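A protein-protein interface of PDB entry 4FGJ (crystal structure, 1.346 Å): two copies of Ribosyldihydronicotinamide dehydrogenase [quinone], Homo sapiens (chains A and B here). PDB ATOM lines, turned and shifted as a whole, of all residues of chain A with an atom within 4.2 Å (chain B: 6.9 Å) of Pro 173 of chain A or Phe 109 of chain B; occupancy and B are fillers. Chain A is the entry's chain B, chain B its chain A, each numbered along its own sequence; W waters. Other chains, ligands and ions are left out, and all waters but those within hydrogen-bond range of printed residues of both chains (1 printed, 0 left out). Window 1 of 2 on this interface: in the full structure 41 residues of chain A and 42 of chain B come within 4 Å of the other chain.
5 positions are printed for both chains.
The backbone carbonyl oxygen (O) of Pro 173 of chain A is in hydrogen-bond range of the side-chain hydroxyl (OG1) of Thr 178 of chain A. N of Gly 177 of chain A sits at hydrogen-bond distance from O of Trp 172 of chain A.
Water W1 lies within hydrogen-bond range of O of Asn 164 of chain B (2.7 Å), O of Asp 166 of chain B (2.8 Å) and NE1 of Trp 172 of chain A (2.9 Å).
Of the 18 printed residues of chain B, 6 touch a printed residue of chain A. Printed residues of chain B that touch a printed residue of chain A: Trp 108, Phe 109, Val 163, Asn 164, Gly 165 and Tyr 169. Hydrophobic or aromatic side chains of chain B that line the printed part of chain A: Trp 108, Phe 109, Val 163 and Tyr 169. Of the 9 printed residues of chain A, 5 touch a printed residue of chain B. Printed residues of chain A that touch a printed residue of chain B: Tyr 135, Trp 172, Pro 173, Gly 177 and Thr 178. Among the printed residues, no Asp or Glu carboxylate lies within 4 Å of a Lys or Arg side-chain nitrogen of the other chain.
The side-chain hydroxyl of Tyr 135 of chain A lies within hydrogen-bond range of the backbone carbonyl oxygen of Val 163 of chain B (3.5 Å). OD1 of Asn 164 of chain B is in hydrogen-bond range of OH of Tyr 135 of chain A, at 2.7 Å.
Among the printed residues, merely in contact across the chains: Gly 177 of chain A with Trp 108 of chain B (3.2 Å), Trp 172 of chain A with Asn 164 of chain B (3.3 Å), Thr 178 of chain A with Trp 108 of chain B (3.4 Å), Trp 172 of chain A with Tyr 169 of chain B (3.4 Å), Trp 172 of chain A with Phe 109 of chain B (3.5 Å), Pro 173 of chain A with Phe 109 of chain B (3.6 Å), Gly 177 of chain A with Phe 109 of chain B (3.7 Å), Tyr 135 of chain A with Phe 109 of chain B (3.7 Å), Pro 173 of chain A with Trp 108 of chain B (3.9 Å) and Trp 172 of chain A with Gly 165 of chain B (3.96 Å).
Pro 173 of chain A touches two residues of chain B. Phe 109 of chain B touches four residues of chain A. Printed residues of chain A within 4 Å of Asn 164 of chain B: Tyr 135 (2.7 Å) and Trp 172 (3.3 Å). Printed residues of chain A within 4 Å of Tyr 169 of chain B: Trp 172. Of the printed residues of chain A, Gly 165 of chain B touches Trp 172. Leu 106 of chain B touches none of the printed residues of chain A. The nearest residue of chain B that does not touch Pro 173 of chain A is Pro 173 of chain B (4.1 Å).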
ATOM      1  N   TYR A 135      14.308  13.472 -13.034  1.00  0.00           N
ATOM      2  CA  TYR A 135      14.519  12.798 -14.325  1.00  0.00           C
ATOM      3  C   TYR A 135      15.697  13.479 -15.030  1.00  0.00           C
ATOM      4  O   TYR A 135      16.762  13.592 -14.422  1.00  0.00           O
ATOM      5  CB  TYR A 135      13.215  12.658 -15.147  1.00  0.00           C
ATOM      6  CG  TYR A 135      12.288  11.611 -14.555  1.00  0.00           C
ATOM      7  CD1 TYR A 135      12.723  10.313 -14.385  1.00  0.00           C
ATOM      8  CD2 TYR A 135      10.976  11.918 -14.174  1.00  0.00           C
ATOM      9  CE1 TYR A 135      11.897   9.340 -13.833  1.00  0.00           C
ATOM     10  CE2 TYR A 135      10.135  10.943 -13.607  1.00  0.00           C
ATOM     11  CZ  TYR A 135      10.611   9.658 -13.447  1.00  0.00           C
ATOM     12  OH  TYR A 135       9.833   8.660 -12.900  1.00  0.00           O
ATOM     13  N   PHE A 170      11.620  -5.979 -14.414  1.00  0.00           N
ATOM     14  CA  PHE A 170      11.918  -5.715 -13.001  1.00  0.00           C
ATOM     15  C   PHE A 170      12.961  -4.613 -12.820  1.00  0.00           C
ATOM     16  O   PHE A 170      13.149  -4.099 -11.727  1.00  0.00           O
ATOM     17  CB  PHE A 170      12.289  -6.998 -12.228  1.00  0.00           C
ATOM     18  CG  PHE A 170      13.624  -7.601 -12.587  1.00  0.00           C
ATOM     19  CD1 PHE A 170      14.807  -6.961 -12.274  1.00  0.00           C
ATOM     20  CD2 PHE A 170      13.688  -8.847 -13.204  1.00  0.00           C
ATOM     21  CE1 PHE A 170      16.016  -7.525 -12.596  1.00  0.00           C
ATOM     22  CE2 PHE A 170      14.893  -9.416 -13.523  1.00  0.00           C
ATOM     23  CZ  PHE A 170      16.061  -8.754 -13.226  1.00  0.00           C
ATOM     24  N   LEU A 171      13.627  -4.215 -13.899  1.00  0.00           N
ATOM     25  CA  LEU A 171      14.588  -3.119 -13.807  1.00  0.00           C
ATOM     26  C   LEU A 171      13.928  -1.750 -13.645  1.00  0.00           C
ATOM     27  O   LEU A 171      14.579  -0.800 -13.197  1.00  0.00           O
ATOM     28  CB  LEU A 171      15.511  -3.100 -15.023  1.00  0.00           C
ATOM     29  CG  LEU A 171      16.398  -4.332 -15.159  1.00  0.00           C
ATOM     30  CD1 LEU A 171      17.118  -4.253 -16.486  1.00  0.00           C
ATOM     31  CD2 LEU A 171      17.404  -4.436 -14.013  1.00  0.00           C
ATOM     32  N   TRP A 172      12.654  -1.644 -14.020  1.00  0.00           N
ATOM     33  CA  TRP A 172      11.981  -0.347 -14.107  1.00  0.00           C
ATOM     34  C   TRP A 172      12.041   0.510 -12.829  1.00  0.00           C
ATOM     35  O   TRP A 172      12.437   1.689 -12.897  1.00  0.00           O
ATOM     36  CB  TRP A 172      10.554  -0.568 -14.614  1.00  0.00           C
ATOM     37  CG  TRP A 172       9.658   0.620 -14.650  1.00  0.00           C
ATOM     38  CD1 TRP A 172       8.631   0.899 -13.787  1.00  0.00           C
ATOM     39  CD2 TRP A 172       9.661   1.663 -15.620  1.00  0.00           C
ATOM     40  NE1 TRP A 172       8.000   2.060 -14.164  1.00  0.00           N
ATOM     41  CE2 TRP A 172       8.624   2.556 -15.280  1.00  0.00           C
ATOM     42  CE3 TRP A 172      10.458   1.941 -16.740  1.00  0.00           C
ATOM     43  CZ2 TRP A 172       8.343   3.689 -16.032  1.00  0.00           C
ATOM     44  CZ3 TRP A 172      10.186   3.071 -17.478  1.00  0.00           C
ATOM     45  CH2 TRP A 172       9.126   3.928 -17.125  1.00  0.00           C
ATOM     46  N   PRO A 173      11.681  -0.059 -11.663  1.00  0.00           N
ATOM     47  CA  PRO A 173      11.696   0.792 -10.451  1.00  0.00           C
ATOM     48  C   PRO A 173      13.101   1.276 -10.100  1.00  0.00           C
ATOM     49  O   PRO A 173      13.247   2.368  -9.553  1.00  0.00           O
ATOM     50  CB  PRO A 173      11.168  -0.140  -9.357  1.00  0.00           C
ATOM     51  CG  PRO A 173      10.314  -1.109 -10.094  1.00  0.00           C
ATOM     52  CD  PRO A 173      11.058  -1.369 -11.392  1.00  0.00           C
ATOM     53  N   LEU A 174      14.110   0.484 -10.457  1.00  0.00           N
ATOM     54  CA  LEU A 174      15.486   0.786 -10.107  1.00  0.00           C
ATOM     55  C   LEU A 174      16.115   1.753 -11.106  1.00  0.00           C
ATOM     56  O   LEU A 174      16.614   2.804 -10.738  1.00  0.00           O
ATOM     57  CB  LEU A 174      16.307  -0.512 -10.039  1.00  0.00           C
ATOM     58  CG  LEU A 174      15.818  -1.556  -9.025  1.00  0.00           C
ATOM     59  CD1 LEU A 174      16.555  -2.872  -9.180  1.00  0.00           C
ATOM     60  CD2 LEU A 174      15.915  -1.006  -7.611  1.00  0.00           C
ATOM     61  N   GLN A 175      16.088   1.386 -12.383  1.00  0.00           N
ATOM     62  CA  GLN A 175      16.700   2.209 -13.420  1.00  0.00           C
ATOM     63  C   GLN A 175      15.926   3.496 -13.644  1.00  0.00           C
ATOM     64  O   GLN A 175      16.500   4.573 -13.676  1.00  0.00           O
ATOM     65  CB  GLN A 175      16.813   1.416 -14.725  1.00  0.00           C
ATOM     66  CG  GLN A 175      17.784   0.253 -14.603  1.00  0.00           C
ATOM     67  CD  GLN A 175      18.126  -0.448 -15.906  1.00  0.00           C
ATOM     68  OE1 GLN A 175      19.191  -1.053 -16.003  1.00  0.00           O
ATOM     69  NE2 GLN A 175      17.261  -0.352 -16.911  1.00  0.00           N
ATOM     70  N   GLY A 177      12.677   4.617 -11.969  1.00  0.00           N
ATOM     71  CA  GLY A 177      12.037   5.242 -10.824  1.00  0.00           C
ATOM     72  C   GLY A 177      13.035   5.822  -9.854  1.00  0.00           C
ATOM     73  O   GLY A 177      12.719   6.783  -9.144  1.00  0.00           O
ATOM     74  N   THR A 178      14.254   5.272  -9.848  1.00  0.00           N
ATOM     75  CA  THR A 178      15.271   5.710  -8.885  1.00  0.00           C
ATOM     76  C   THR A 178      16.418   6.416  -9.583  1.00  0.00           C
ATOM     77  O   THR A 178      16.601   7.621  -9.417  1.00  0.00           O
ATOM     78  CB  THR A 178      15.796   4.534  -8.041  1.00  0.00           C
ATOM     79  OG1 THR A 178      14.676   3.835  -7.472  1.00  0.00           O
ATOM     80  CG2 THR A 178      16.698   5.017  -6.898  1.00  0.00           C
ATOM     81  N   PHE B 104       1.563   0.954   2.958  1.00  0.00           N
ATOM     82  CA  PHE B 104       2.836   1.669   2.892  1.00  0.00           C
ATOM     83  C   PHE B 104       2.818   2.837   1.930  1.00  0.00           C
ATOM     84  O   PHE B 104       2.092   2.812   0.927  1.00  0.00           O
ATOM     85  CB  PHE B 104       3.974   0.720   2.448  1.00  0.00           C
ATOM     86  CG  PHE B 104       3.743   0.092   1.101  1.00  0.00           C
ATOM     87  CD1 PHE B 104       2.928  -1.014   0.957  1.00  0.00           C
ATOM     88  CD2 PHE B 104       4.365   0.602  -0.031  1.00  0.00           C
ATOM     89  CE1 PHE B 104       2.701  -1.583  -0.290  1.00  0.00           C
ATOM     90  CE2 PHE B 104       4.156   0.029  -1.270  1.00  0.00           C
ATOM     91  CZ  PHE B 104       3.335  -1.067  -1.397  1.00  0.00           C
ATOM     92  N   LEU B 106       4.781   4.659  -1.076  1.00  0.00           N
ATOM     93  CA  LEU B 106       5.713   4.287  -2.139  1.00  0.00           C
ATOM     94  C   LEU B 106       7.050   4.971  -1.896  1.00  0.00           C
ATOM     95  O   LEU B 106       7.105   6.194  -1.737  1.00  0.00           O
ATOM     96  CB  LEU B 106       5.152   4.714  -3.492  1.00  0.00           C
ATOM     97  CG  LEU B 106       5.758   4.074  -4.742  1.00  0.00           C
ATOM     98  CD1 LEU B 106       5.467   2.606  -4.810  1.00  0.00           C
ATOM     99  CD2 LEU B 106       5.264   4.794  -6.015  1.00  0.00           C
ATOM    100  N   TYR B 107       8.114   4.168  -1.817  1.00  0.00           N
ATOM    101  CA  TYR B 107       9.485   4.667  -1.708  1.00  0.00           C
ATOM    102  C   TYR B 107      10.242   4.124  -2.930  1.00  0.00           C
ATOM    103  O   TYR B 107      10.416   2.901  -3.061  1.00  0.00           O
ATOM    104  CB  TYR B 107      10.185   4.135  -0.447  1.00  0.00           C
ATOM    105  CG  TYR B 107       9.980   4.871   0.862  1.00  0.00           C
ATOM    106  CD1 TYR B 107       8.918   5.735   1.084  1.00  0.00           C
ATOM    107  CD2 TYR B 107      10.890   4.678   1.901  1.00  0.00           C
ATOM    108  CE1 TYR B 107       8.776   6.383   2.303  1.00  0.00           C
ATOM    109  CE2 TYR B 107      10.768   5.307   3.095  1.00  0.00           C
ATOM    110  CZ  TYR B 107       9.717   6.166   3.305  1.00  0.00           C
ATOM    111  OH  TYR B 107       9.637   6.792   4.538  1.00  0.00           O
ATOM    112  N   TRP B 108      10.683   5.014  -3.814  1.00  0.00           N
ATOM    113  CA  TRP B 108      11.449   4.618  -4.990  1.00  0.00           C
ATOM    114  C   TRP B 108      10.762   3.498  -5.778  1.00  0.00           C
ATOM    115  O   TRP B 108      11.354   2.485  -6.138  1.00  0.00           O
ATOM    116  CB  TRP B 108      12.892   4.270  -4.597  1.00  0.00           C
ATOM    117  CG  TRP B 108      13.678   5.445  -4.113  1.00  0.00           C
ATOM    118  CD1 TRP B 108      14.316   5.578  -2.900  1.00  0.00           C
ATOM    119  CD2 TRP B 108      13.911   6.668  -4.821  1.00  0.00           C
ATOM    120  NE1 TRP B 108      14.927   6.810  -2.820  1.00  0.00           N
ATOM    121  CE2 TRP B 108      14.717   7.485  -3.995  1.00  0.00           C
ATOM    122  CE3 TRP B 108      13.553   7.138  -6.088  1.00  0.00           C
ATOM    123  CZ2 TRP B 108      15.148   8.747  -4.392  1.00  0.00           C
ATOM    124  CZ3 TRP B 108      14.004   8.388  -6.478  1.00  0.00           C
ATOM    125  CH2 TRP B 108      14.786   9.175  -5.631  1.00  0.00           C
ATOM    126  N   PHE B 109       9.478   3.739  -6.072  1.00  0.00           N
ATOM    127  CA  PHE B 109       8.686   2.860  -6.939  1.00  0.00           C
ATOM    128  C   PHE B 109       8.584   1.469  -6.312  1.00  0.00           C
ATOM    129  O   PHE B 109       8.397   0.486  -7.019  1.00  0.00           O
ATOM    130  CB  PHE B 109       9.291   2.727  -8.356  1.00  0.00           C
ATOM    131  CG  PHE B 109       8.907   3.809  -9.340  1.00  0.00           C
ATOM    132  CD1 PHE B 109       8.673   5.114  -8.965  1.00  0.00           C
ATOM    133  CD2 PHE B 109       8.802   3.480 -10.687  1.00  0.00           C
ATOM    134  CE1 PHE B 109       8.352   6.084  -9.935  1.00  0.00           C
ATOM    135  CE2 PHE B 109       8.483   4.435 -11.637  1.00  0.00           C
ATOM    136  CZ  PHE B 109       8.253   5.734 -11.250  1.00  0.00           C
ATOM    137  N   SER B 110       8.678   1.388  -4.986  1.00  0.00           N
ATOM    138  CA  SER B 110       8.685   0.114  -4.290  1.00  0.00           C
ATOM    139  C   SER B 110       8.247   0.320  -2.847  1.00  0.00           C
ATOM    140  O   SER B 110       7.661   1.344  -2.512  1.00  0.00           O
ATOM    141  CB  SER B 110      10.085  -0.508  -4.401  1.00  0.00           C
ATOM    142  OG  SER B 110      10.178  -1.789  -3.816  1.00  0.00           O
ATOM    143  N   VAL B 111       8.495  -0.681  -2.007  1.00  0.00           N
ATOM    144  CA  VAL B 111       8.168  -0.610  -0.591  1.00  0.00           C
ATOM    145  C   VAL B 111       9.333   0.040   0.159  1.00  0.00           C
ATOM    146  O   VAL B 111      10.496  -0.084  -0.233  1.00  0.00           O
ATOM    147  CB  VAL B 111       7.911  -2.008  -0.008  1.00  0.00           C
ATOM    148  CG1 VAL B 111       6.618  -2.570  -0.548  1.00  0.00           C
ATOM    149  CG2 VAL B 111       9.066  -2.973  -0.296  1.00  0.00           C
ATOM    150  N   TYR B 158       1.317   8.796 -13.192  1.00  0.00           N
ATOM    151  CA  TYR B 158       1.362   7.350 -13.263  1.00  0.00           C
ATOM    152  C   TYR B 158       0.474   6.797 -14.377  1.00  0.00           C
ATOM    153  O   TYR B 158      -0.325   5.892 -14.162  1.00  0.00           O
ATOM    154  CB  TYR B 158       0.997   6.752 -11.901  1.00  0.00           C
ATOM    155  CG  TYR B 158       2.121   6.915 -10.892  1.00  0.00           C
ATOM    156  CD1 TYR B 158       3.268   6.130 -10.978  1.00  0.00           C
ATOM    157  CD2 TYR B 158       2.056   7.876  -9.888  1.00  0.00           C
ATOM    158  CE1 TYR B 158       4.306   6.267 -10.064  1.00  0.00           C
ATOM    159  CE2 TYR B 158       3.094   8.022  -8.963  1.00  0.00           C
ATOM    160  CZ  TYR B 158       4.214   7.217  -9.070  1.00  0.00           C
ATOM    161  OH  TYR B 158       5.266   7.346  -8.195  1.00  0.00           O
ATOM    162  N   VAL B 163       5.187  10.720 -16.876  1.00  0.00           N
ATOM    163  CA  VAL B 163       6.624  10.676 -16.564  1.00  0.00           C
ATOM    164  C   VAL B 163       7.023   9.443 -15.776  1.00  0.00           C
ATOM    165  O   VAL B 163       8.153   8.936 -15.930  1.00  0.00           O
ATOM    166  CB  VAL B 163       7.119  11.925 -15.795  1.00  0.00           C
ATOM    167  CG1 VAL B 163       7.083  13.157 -16.711  1.00  0.00           C
ATOM    168  CG2 VAL B 163       6.336  12.124 -14.489  1.00  0.00           C
ATOM    169  N   ASN B 164       6.114   8.969 -14.931  1.00  0.00           N
ATOM    170  CA  ASN B 164       6.407   7.832 -14.081  1.00  0.00           C
ATOM    171  C   ASN B 164       6.006   6.504 -14.696  1.00  0.00           C
ATOM    172  O   ASN B 164       6.331   5.453 -14.148  1.00  0.00           O
ATOM    173  CB  ASN B 164       5.715   7.982 -12.712  1.00  0.00           C
ATOM    174  CG  ASN B 164       6.281   9.126 -11.873  1.00  0.00           C
ATOM    175  OD1 ASN B 164       7.450   9.530 -12.020  1.00  0.00           O
ATOM    176  ND2 ASN B 164       5.456   9.627 -10.948  1.00  0.00           N
ATOM    177  N   GLY B 165       5.305   6.534 -15.836  1.00  0.00           N
ATOM    178  CA  GLY B 165       4.748   5.314 -16.382  1.00  0.00           C
ATOM    179  C   GLY B 165       3.519   4.862 -15.603  1.00  0.00           C
ATOM    180  O   GLY B 165       3.191   5.411 -14.554  1.00  0.00           O
ATOM    181  N   ASP B 166       2.847   3.838 -16.113  1.00  0.00           N
ATOM    182  CA  ASP B 166       1.653   3.286 -15.458  1.00  0.00           C
ATOM    183  C   ASP B 166       1.997   2.780 -14.054  1.00  0.00           C
ATOM    184  O   ASP B 166       3.054   2.180 -13.862  1.00  0.00           O
ATOM    185  CB  ASP B 166       1.123   2.116 -16.301  1.00  0.00           C
ATOM    186  CG  ASP B 166      -0.303   1.706 -15.944  1.00  0.00           C
ATOM    187  OD1 ASP B 166      -0.762   1.975 -14.828  1.00  0.00           O
ATOM    188  OD2 ASP B 166      -0.955   1.087 -16.806  1.00  0.00           O
ATOM    189  N   TYR B 169       3.219  -0.706 -13.793  1.00  0.00           N
ATOM    190  CA  TYR B 169       4.613  -1.029 -14.062  1.00  0.00           C
ATOM    191  C   TYR B 169       5.403  -1.243 -12.775  1.00  0.00           C
ATOM    192  O   TYR B 169       6.219  -2.154 -12.697  1.00  0.00           O
ATOM    193  CB  TYR B 169       5.283   0.078 -14.876  1.00  0.00           C
ATOM    194  CG  TYR B 169       4.724   0.331 -16.262  1.00  0.00           C
ATOM    195  CD1 TYR B 169       3.834  -0.547 -16.869  1.00  0.00           C
ATOM    196  CD2 TYR B 169       5.114   1.460 -16.964  1.00  0.00           C
ATOM    197  CE1 TYR B 169       3.345  -0.295 -18.134  1.00  0.00           C
ATOM    198  CE2 TYR B 169       4.625   1.720 -18.228  1.00  0.00           C
ATOM    199  CZ  TYR B 169       3.742   0.842 -18.805  1.00  0.00           C
ATOM    200  OH  TYR B 169       3.264   1.106 -20.074  1.00  0.00           O
ATOM    201  N   PHE B 170       5.180  -0.419 -11.753  1.00  0.00           N
ATOM    202  CA  PHE B 170       5.944  -0.604 -10.513  1.00  0.00           C
ATOM    203  C   PHE B 170       5.352  -1.701  -9.647  1.00  0.00           C
ATOM    204  O   PHE B 170       6.006  -2.230  -8.762  1.00  0.00           O
ATOM    205  CB  PHE B 170       6.159   0.705  -9.719  1.00  0.00           C
ATOM    206  CG  PHE B 170       4.919   1.268  -9.043  1.00  0.00           C
ATOM    207  CD1 PHE B 170       4.297   0.618  -7.977  1.00  0.00           C
ATOM    208  CD2 PHE B 170       4.406   2.485  -9.452  1.00  0.00           C
ATOM    209  CE1 PHE B 170       3.181   1.165  -7.355  1.00  0.00           C
ATOM    210  CE2 PHE B 170       3.293   3.032  -8.840  1.00  0.00           C
ATOM    211  CZ  PHE B 170       2.678   2.371  -7.785  1.00  0.00           C
ATOM    212  N   LEU B 171       4.119  -2.084  -9.923  1.00  0.00           N
ATOM    213  CA  LEU B 171       3.484  -3.137  -9.140  1.00  0.00           C
ATOM    214  C   LEU B 171       4.070  -4.515  -9.441  1.00  0.00           C
ATOM    215  O   LEU B 171       4.017  -5.409  -8.618  1.00  0.00           O
ATOM    216  CB  LEU B 171       1.970  -3.139  -9.381  1.00  0.00           C
ATOM    217  CG  LEU B 171       1.218  -1.973  -8.751  1.00  0.00           C
ATOM    218  CD1 LEU B 171      -0.220  -1.960  -9.251  1.00  0.00           C
ATOM    219  CD2 LEU B 171       1.251  -2.039  -7.216  1.00  0.00           C
ATOM    220  N   TRP B 172       4.662  -4.677 -10.620  1.00  0.00           N
ATOM    221  CA  TRP B 172       5.108  -5.990 -11.082  1.00  0.00           C
ATOM    222  C   TRP B 172       5.997  -6.749 -10.093  1.00  0.00           C
ATOM    223  O   TRP B 172       5.706  -7.895  -9.777  1.00  0.00           O
ATOM    224  CB  TRP B 172       5.754  -5.833 -12.463  1.00  0.00           C
ATOM    225  CG  TRP B 172       6.371  -7.027 -13.058  1.00  0.00           C
ATOM    226  CD1 TRP B 172       7.712  -7.264 -13.213  1.00  0.00           C
ATOM    227  CD2 TRP B 172       5.697  -8.131 -13.658  1.00  0.00           C
ATOM    228  NE1 TRP B 172       7.911  -8.447 -13.874  1.00  0.00           N
ATOM    229  CE2 TRP B 172       6.690  -9.000 -14.165  1.00  0.00           C
ATOM    230  CE3 TRP B 172       4.351  -8.475 -13.822  1.00  0.00           C
ATOM    231  CZ2 TRP B 172       6.378 -10.196 -14.805  1.00  0.00           C
ATOM    232  CZ3 TRP B 172       4.044  -9.659 -14.468  1.00  0.00           C
ATOM    233  CH2 TRP B 172       5.059 -10.502 -14.960  1.00  0.00           C
ATOM    234  N   PRO B 173       7.088  -6.130  -9.604  1.00  0.00           N
ATOM    235  CA  PRO B 173       7.946  -6.883  -8.680  1.00  0.00           C
ATOM    236  C   PRO B 173       7.234  -7.293  -7.397  1.00  0.00           C
ATOM    237  O   PRO B 173       7.564  -8.323  -6.841  1.00  0.00           O
ATOM    238  CB  PRO B 173       9.070  -5.892  -8.360  1.00  0.00           C
ATOM    239  CG  PRO B 173       9.109  -5.020  -9.570  1.00  0.00           C
ATOM    240  CD  PRO B 173       7.680  -4.829  -9.955  1.00  0.00           C
ATOM    241  N   LEU B 174       6.297  -6.468  -6.953  1.00  0.00           N
ATOM    242  CA  LEU B 174       5.577  -6.710  -5.701  1.00  0.00           C
ATOM    243  C   LEU B 174       4.441  -7.729  -5.883  1.00  0.00           C
ATOM    244  O   LEU B 174       4.389  -8.751  -5.198  1.00  0.00           O
ATOM    245  CB  LEU B 174       5.028  -5.389  -5.181  1.00  0.00           C
ATOM    246  CG  LEU B 174       6.103  -4.342  -4.846  1.00  0.00           C
ATOM    247  CD1 LEU B 174       5.481  -2.995  -4.521  1.00  0.00           C
ATOM    248  CD2 LEU B 174       6.969  -4.828  -3.700  1.00  0.00           C
HETATM  249  O   HOH W   1       5.581   3.111 -12.961  1.00  0.00           O
